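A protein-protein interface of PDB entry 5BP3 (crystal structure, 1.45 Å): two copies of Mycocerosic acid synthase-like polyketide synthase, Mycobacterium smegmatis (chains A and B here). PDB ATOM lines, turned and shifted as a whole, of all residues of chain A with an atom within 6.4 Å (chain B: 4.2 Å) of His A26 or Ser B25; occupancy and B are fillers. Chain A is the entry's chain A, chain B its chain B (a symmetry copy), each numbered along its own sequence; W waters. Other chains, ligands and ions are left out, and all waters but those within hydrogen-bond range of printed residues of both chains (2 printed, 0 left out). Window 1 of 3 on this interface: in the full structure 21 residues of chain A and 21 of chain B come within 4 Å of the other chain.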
ATOM      1  N   VAL A  17     -32.142  -9.386 -23.920  1.00  0.00           N
ATOM      2  CA  VAL A  17     -31.561 -10.701 -23.689  1.00  0.00           C
ATOM      3  C   VAL A  17     -32.722 -11.687 -23.575  1.00  0.00           C
ATOM      4  O   VAL A  17     -33.764 -11.370 -23.002  1.00  0.00           O
ATOM      5  CB  VAL A  17     -30.692 -10.709 -22.399  1.00  0.00           C
ATOM      6  CG1 VAL A  17     -30.120 -12.072 -22.118  1.00  0.00           C
ATOM      7  CG2 VAL A  17     -29.543  -9.678 -22.526  1.00  0.00           C
ATOM      8  N   VAL A  19     -34.676 -14.804 -22.025  1.00  0.00           N
ATOM      9  CA  VAL A  19     -34.712 -15.350 -20.680  1.00  0.00           C
ATOM     10  C   VAL A  19     -35.619 -16.562 -20.672  1.00  0.00           C
ATOM     11  O   VAL A  19     -36.522 -16.687 -21.498  1.00  0.00           O
ATOM     12  CB  VAL A  19     -35.237 -14.364 -19.634  1.00  0.00           C
ATOM     13  CG1 VAL A  19     -34.302 -13.148 -19.513  1.00  0.00           C
ATOM     14  CG2 VAL A  19     -36.612 -13.885 -19.981  1.00  0.00           C
ATOM     15  N   LEU A  23     -37.331 -18.695 -14.885  1.00  0.00           N
ATOM     16  CA  LEU A  23     -36.121 -18.297 -14.161  1.00  0.00           C
ATOM     17  C   LEU A  23     -35.860 -16.776 -14.259  1.00  0.00           C
ATOM     18  O   LEU A  23     -35.401 -16.185 -13.312  1.00  0.00           O
ATOM     19  CB  LEU A  23     -34.901 -19.031 -14.673  1.00  0.00           C
ATOM     20  CG  LEU A  23     -34.891 -20.561 -14.541  1.00  0.00           C
ATOM     21  CD1 LEU A  23     -33.600 -21.046 -15.153  1.00  0.00           C
ATOM     22  CD2 LEU A  23     -34.979 -20.980 -13.104  1.00  0.00           C
ATOM     23  N   GLY A  24     -36.180 -16.180 -15.393  1.00  0.00           N
ATOM     24  CA  GLY A  24     -35.955 -14.738 -15.545  1.00  0.00           C
ATOM     25  C   GLY A  24     -34.504 -14.319 -15.657  1.00  0.00           C
ATOM     26  O   GLY A  24     -33.662 -14.995 -16.248  1.00  0.00           O
ATOM     27  N   SER A  25     -34.212 -13.166 -15.061  1.00  0.00           N
ATOM     28  CA  SER A  25     -32.910 -12.528 -15.305  1.00  0.00           C
ATOM     29  C   SER A  25     -31.827 -13.260 -14.544  1.00  0.00           C
ATOM     30  O   SER A  25     -32.033 -13.605 -13.378  1.00  0.00           O
ATOM     31  CB  SER A  25     -32.937 -11.071 -14.853  1.00  0.00           C
ATOM     32  OG  SER A  25     -33.705 -10.310 -15.759  1.00  0.00           O
ATOM     33  N   HIS A  26     -30.695 -13.484 -15.215  1.00  0.00           N
ATOM     34  CA  HIS A  26     -29.606 -14.324 -14.752  1.00  0.00           C
ATOM     35  C   HIS A  26     -28.304 -13.546 -14.555  1.00  0.00           C
ATOM     36  O   HIS A  26     -27.912 -12.772 -15.449  1.00  0.00           O
ATOM     37  CB  HIS A  26     -29.367 -15.361 -15.840  1.00  0.00           C
ATOM     38  CG  HIS A  26     -28.221 -16.279 -15.577  1.00  0.00           C
ATOM     39  ND1 HIS A  26     -27.331 -16.655 -16.562  1.00  0.00           N
ATOM     40  CD2 HIS A  26     -27.786 -16.861 -14.437  1.00  0.00           C
ATOM     41  CE1 HIS A  26     -26.445 -17.496 -16.050  1.00  0.00           C
ATOM     42  NE2 HIS A  26     -26.694 -17.628 -14.761  1.00  0.00           N
ATOM     43  N   VAL A  27     -27.662 -13.723 -13.414  1.00  0.00           N
ATOM     44  CA  VAL A  27     -26.288 -13.213 -13.225  1.00  0.00           C
ATOM     45  C   VAL A  27     -25.427 -14.289 -12.583  1.00  0.00           C
ATOM     46  O   VAL A  27     -25.943 -15.252 -12.000  1.00  0.00           O
ATOM     47  CB  VAL A  27     -26.251 -11.959 -12.339  1.00  0.00           C
ATOM     48  CG1 VAL A  27     -27.045 -10.822 -12.978  1.00  0.00           C
ATOM     49  CG2 VAL A  27     -26.798 -12.250 -10.952  1.00  0.00           C
ATOM     50  N   VAL A  28     -24.121 -14.178 -12.768  1.00  0.00           N
ATOM     51  CA  VAL A  28     -23.154 -14.933 -12.002  1.00  0.00           C
ATOM     52  C   VAL A  28     -22.641 -14.002 -10.912  1.00  0.00           C
ATOM     53  O   VAL A  28     -22.364 -12.834 -11.191  1.00  0.00           O
ATOM     54  CB  VAL A  28     -22.040 -15.401 -12.911  1.00  0.00           C
ATOM     55  CG1 VAL A  28     -20.934 -16.032 -12.116  1.00  0.00           C
ATOM     56  CG2 VAL A  28     -22.588 -16.369 -13.942  1.00  0.00           C
ATOM     57  N   HIS A  36     -24.529 -18.893  -9.425  1.00  0.00           N
ATOM     58  CA  HIS A  36     -25.501 -18.278 -10.296  1.00  0.00           C
ATOM     59  C   HIS A  36     -26.722 -17.829  -9.494  1.00  0.00           C
ATOM     60  O   HIS A  36     -27.129 -18.484  -8.533  1.00  0.00           O
ATOM     61  CB  HIS A  36     -25.961 -19.282 -11.372  1.00  0.00           C
ATOM     62  CG  HIS A  36     -24.864 -19.726 -12.286  1.00  0.00           C
ATOM     63  ND1 HIS A  36     -24.835 -19.399 -13.625  1.00  0.00           N
ATOM     64  CD2 HIS A  36     -23.752 -20.465 -12.054  1.00  0.00           C
ATOM     65  CE1 HIS A  36     -23.741 -19.900 -14.175  1.00  0.00           C
ATOM     66  NE2 HIS A  36     -23.070 -20.557 -13.245  1.00  0.00           N
ATOM     67  N   LEU A  37     -27.334 -16.746  -9.935  1.00  0.00           N
ATOM     68  CA  LEU A  37     -28.530 -16.209  -9.330  1.00  0.00           C
ATOM     69  C   LEU A  37     -29.479 -15.758 -10.429  1.00  0.00           C
ATOM     70  O   LEU A  37     -29.102 -15.026 -11.351  1.00  0.00           O
ATOM     71  CB  LEU A  37     -28.234 -15.054  -8.354  1.00  0.00           C
ATOM     72  CG  LEU A  37     -29.416 -14.394  -7.650  1.00  0.00           C
ATOM     73  CD1 LEU A  37     -30.162 -15.374  -6.766  1.00  0.00           C
ATOM     74  CD2 LEU A  37     -28.987 -13.184  -6.813  1.00  0.00           C
ATOM     75  N   TRP A  38     -30.732 -16.201 -10.323  1.00  0.00           N
ATOM     76  CA  TRP A  38     -31.771 -15.742 -11.201  1.00  0.00           C
ATOM     77  C   TRP A  38     -32.876 -15.068 -10.382  1.00  0.00           C
ATOM     78  O   TRP A  38     -33.188 -15.504  -9.263  1.00  0.00           O
ATOM     79  CB  TRP A  38     -32.431 -16.898 -11.953  1.00  0.00           C
ATOM     80  CG  TRP A  38     -31.649 -17.644 -12.975  1.00  0.00           C
ATOM     81  CD1 TRP A  38     -31.729 -17.505 -14.322  1.00  0.00           C
ATOM     82  CD2 TRP A  38     -30.766 -18.755 -12.737  1.00  0.00           C
ATOM     83  NE1 TRP A  38     -30.923 -18.432 -14.938  1.00  0.00           N
ATOM     84  CE2 TRP A  38     -30.325 -19.209 -13.984  1.00  0.00           C
ATOM     85  CE3 TRP A  38     -30.307 -19.400 -11.583  1.00  0.00           C
ATOM     86  CZ2 TRP A  38     -29.458 -20.297 -14.119  1.00  0.00           C
ATOM     87  CZ3 TRP A  38     -29.450 -20.469 -11.719  1.00  0.00           C
ATOM     88  CH2 TRP A  38     -29.025 -20.899 -12.978  1.00  0.00           C
ATOM     89  N   GLN A  39     -33.512 -14.044 -10.952  1.00  0.00           N
ATOM     90  CA  GLN A  39     -34.731 -13.482 -10.382  1.00  0.00           C
ATOM     91  C   GLN A  39     -35.845 -13.556 -11.409  1.00  0.00           C
ATOM     92  O   GLN A  39     -35.775 -12.941 -12.479  1.00  0.00           O
ATOM     93  CB  GLN A  39     -34.552 -12.006  -9.949  1.00  0.00           C
ATOM     94  CG  GLN A  39     -35.803 -11.512  -9.248  1.00  0.00           C
ATOM     95  CD  GLN A  39     -35.769 -10.031  -8.946  1.00  0.00           C
ATOM     96  OE1 GLN A  39     -34.717  -9.406  -9.012  1.00  0.00           O
ATOM     97  NE2 GLN A  39     -36.918  -9.468  -8.614  1.00  0.00           N
ATOM     98  N   PRO A  76     -26.886 -23.710 -18.350  1.00  0.00           N
ATOM     99  CA  PRO A  76     -26.133 -22.484 -18.017  1.00  0.00           C
ATOM    100  C   PRO A  76     -25.072 -22.684 -16.938  1.00  0.00           C
ATOM    101  O   PRO A  76     -24.043 -22.009 -16.959  1.00  0.00           O
ATOM    102  CB  PRO A  76     -27.211 -21.530 -17.483  1.00  0.00           C
ATOM    103  CG  PRO A  76     -28.489 -22.066 -17.935  1.00  0.00           C
ATOM    104  CD  PRO A  76     -28.338 -23.515 -18.241  1.00  0.00           C
ATOM    105  N   VAL A  77     -25.312 -23.606 -16.010  1.00  0.00           N
ATOM    106  CA  VAL A  77     -24.423 -23.802 -14.874  1.00  0.00           C
ATOM    107  C   VAL A  77     -23.287 -24.767 -15.159  1.00  0.00           C
ATOM    108  O   VAL A  77     -22.133 -24.511 -14.800  1.00  0.00           O
ATOM    109  CB  VAL A  77     -25.201 -24.269 -13.625  1.00  0.00           C
ATOM    110  CG1 VAL A  77     -24.232 -24.528 -12.463  1.00  0.00           C
ATOM    111  CG2 VAL A  77     -26.203 -23.194 -13.230  1.00  0.00           C
ATOM    112  N   LEU B  23     -24.791  -1.924 -18.295  1.00  0.00           N
ATOM    113  CA  LEU B  23     -25.047  -2.573 -17.014  1.00  0.00           C
ATOM    114  C   LEU B  23     -25.394  -4.048 -17.230  1.00  0.00           C
ATOM    115  O   LEU B  23     -25.009  -4.893 -16.441  1.00  0.00           O
ATOM    116  CB  LEU B  23     -26.175  -1.882 -16.263  1.00  0.00           C
ATOM    117  CG  LEU B  23     -25.945  -0.436 -15.787  1.00  0.00           C
ATOM    118  CD1 LEU B  23     -27.235  -0.009 -15.112  1.00  0.00           C
ATOM    119  CD2 LEU B  23     -24.793  -0.359 -14.815  1.00  0.00           C
ATOM    120  N   GLY B  24     -26.106  -4.357 -18.301  1.00  0.00           N
ATOM    121  CA  GLY B  24     -26.494  -5.758 -18.520  1.00  0.00           C
ATOM    122  C   GLY B  24     -27.581  -6.274 -17.599  1.00  0.00           C
ATOM    123  O   GLY B  24     -28.474  -5.552 -17.187  1.00  0.00           O
ATOM    124  N   SER B  25     -27.491  -7.573 -17.319  1.00  0.00           N
ATOM    125  CA  SER B  25     -28.562  -8.272 -16.604  1.00  0.00           C
ATOM    126  C   SER B  25     -28.665  -7.803 -15.171  1.00  0.00           C
ATOM    127  O   SER B  25     -27.647  -7.661 -14.487  1.00  0.00           O
ATOM    128  CB  SER B  25     -28.283  -9.779 -16.632  1.00  0.00           C
ATOM    129  OG  SER B  25     -28.464 -10.298 -17.931  1.00  0.00           O
ATOM    130  N   HIS B  26     -29.900  -7.585 -14.723  1.00  0.00           N
ATOM    131  CA  HIS B  26     -30.207  -6.954 -13.452  1.00  0.00           C
ATOM    132  C   HIS B  26     -31.005  -7.892 -12.559  1.00  0.00           C
ATOM    133  O   HIS B  26     -32.015  -8.426 -12.992  1.00  0.00           O
ATOM    134  CB  HIS B  26     -31.083  -5.728 -13.732  1.00  0.00           C
ATOM    135  CG  HIS B  26     -31.599  -5.031 -12.515  1.00  0.00           C
ATOM    136  ND1 HIS B  26     -32.895  -4.574 -12.425  1.00  0.00           N
ATOM    137  CD2 HIS B  26     -30.997  -4.679 -11.354  1.00  0.00           C
ATOM    138  CE1 HIS B  26     -33.069  -3.966 -11.264  1.00  0.00           C
ATOM    139  NE2 HIS B  26     -31.932  -4.014 -10.597  1.00  0.00           N
ATOM    140  N   LEU B  37     -27.914  -5.844  -8.142  1.00  0.00           N
ATOM    141  CA  LEU B  37     -26.708  -6.359  -8.779  1.00  0.00           C
ATOM    142  C   LEU B  37     -26.939  -6.442 -10.294  1.00  0.00           C
ATOM    143  O   LEU B  37     -27.957  -6.973 -10.770  1.00  0.00           O
ATOM    144  CB  LEU B  37     -26.322  -7.728  -8.192  1.00  0.00           C
ATOM    145  CG  LEU B  37     -25.080  -8.367  -8.783  1.00  0.00           C
ATOM    146  CD1 LEU B  37     -23.838  -7.490  -8.504  1.00  0.00           C
ATOM    147  CD2 LEU B  37     -24.913  -9.802  -8.230  1.00  0.00           C
ATOM    148  N   TRP B  38     -26.007  -5.863 -11.062  1.00  0.00           N
ATOM    149  CA  TRP B  38     -25.982  -6.032 -12.499  1.00  0.00           C
ATOM    150  C   TRP B  38     -24.703  -6.744 -12.901  1.00  0.00           C
ATOM    151  O   TRP B  38     -23.635  -6.474 -12.329  1.00  0.00           O
ATOM    152  CB  TRP B  38     -25.968  -4.683 -13.221  1.00  0.00           C
ATOM    153  CG  TRP B  38     -27.170  -3.877 -13.112  1.00  0.00           C
ATOM    154  CD1 TRP B  38     -28.147  -3.759 -14.036  1.00  0.00           C
ATOM    155  CD2 TRP B  38     -27.497  -2.965 -12.056  1.00  0.00           C
ATOM    156  NE1 TRP B  38     -29.076  -2.844 -13.621  1.00  0.00           N
ATOM    157  CE2 TRP B  38     -28.709  -2.350 -12.403  1.00  0.00           C
ATOM    158  CE3 TRP B  38     -26.893  -2.627 -10.847  1.00  0.00           C
ATOM    159  CZ2 TRP B  38     -29.327  -1.392 -11.589  1.00  0.00           C
ATOM    160  CZ3 TRP B  38     -27.504  -1.659 -10.036  1.00  0.00           C
ATOM    161  CH2 TRP B  38     -28.700  -1.057 -10.413  1.00  0.00           C
ATOM    162  N   GLN B  39     -24.785  -7.586 -13.921  1.00  0.00           N
ATOM    163  CA  GLN B  39     -23.596  -8.169 -14.548  1.00  0.00           C
ATOM    164  C   GLN B  39     -23.562  -7.798 -16.016  1.00  0.00           C
ATOM    165  O   GLN B  39     -24.423  -8.160 -16.797  1.00  0.00           O
ATOM    166  CB  GLN B  39     -23.568  -9.702 -14.405  1.00  0.00           C
ATOM    167  CG  GLN B  39     -22.270 -10.276 -14.973  1.00  0.00           C
ATOM    168  CD  GLN B  39     -22.284 -11.751 -15.143  1.00  0.00           C
ATOM    169  OE1 GLN B  39     -23.192 -12.419 -14.689  1.00  0.00           O
ATOM    170  NE2 GLN B  39     -21.286 -12.273 -15.828  1.00  0.00           N
HETATM  171  O   HOH W   1     -32.122  -7.928 -16.460  1.00  0.00           O
HETATM  172  O   HOH W   2     -30.553 -12.808 -18.153  1.00  0.00           O
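The backbone NH (N) of Val A28 lies within hydrogen-bond range of the side-chain amide oxygen (OE1) of Gln B39 (2.8 Å).
The backbone NH (N) of Gln A39 sits at hydrogen-bond distance from the backbone carbonyl oxygen (O) of Ser A25, 2.9 Å away. A ring nitrogen (NE2) of His A26 is in hydrogen-bond range of a ring nitrogen (ND1) of His A36, at 2.8 Å. The backbone NH of Val A27 lies within hydrogen-bond range of the backbone carbonyl oxygen of Leu A37 (2.8 Å). The backbone NH (N) of Gln B39 is in hydrogen-bond range of the backbone carbonyl oxygen (O) of Ser B25 (2.9 Å).
His B26 touches Ser A25 (O to CB, 3.4 Å). His A26 touches Ser B25 (O to CB, 3.2 Å). Val A27 touches Ser B25 (CG1 to O, 3.6 Å). CA of Val A27 touches OE1 of Gln B39 (3.5 Å).
Of the printed residues of chain B, Ser A25 touches His B26 (3.4 Å). Of chain B, only Ser B25 (3.2 Å) comes within 4 Å of His A26. Printed residues of chain B within 4 Å of Val A27: Ser B25 (3.6 Å) and Gln B39 (3.5 Å). Leu A37 touches none of the printed residues of chain B. Of chain A, only His A26 (3.2 Å) and Val A27 (3.6 Å) come within 4 Å of Ser B25. Printed residues of chain A within 4 Å of Gln B39: Val A27 (3.5 Å) and Val A28 (2.8 Å). The nearest printed residue of chain A that does not touch His B26 is Val A27 (4.7 Å).
Of the 7 printed residues of chain B, 3 touch a printed residue of chain A. Along chain B the printed residues that touch a printed residue of chain A span positions 25 to 39. Among the printed residues, 5 pairs touch across the chains.
Ser A25 touches His B26, and with the chains exchanged His A26 touches Ser B25. Positions printed for both chains: 23, 24, 25, 26, 37, 38 and 39. Of the 5 pairs that touch across the chains among the printed residues, 2 have their exchanged pair printed and touching as well.
Water W1 bridges N of His B26 (2.8 Å) and OG of Ser A25 (2.9 Å). Water W2 bridges the backbone NH (N) of His A26 and the side-chain hydroxyl (OG) of Ser B25.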
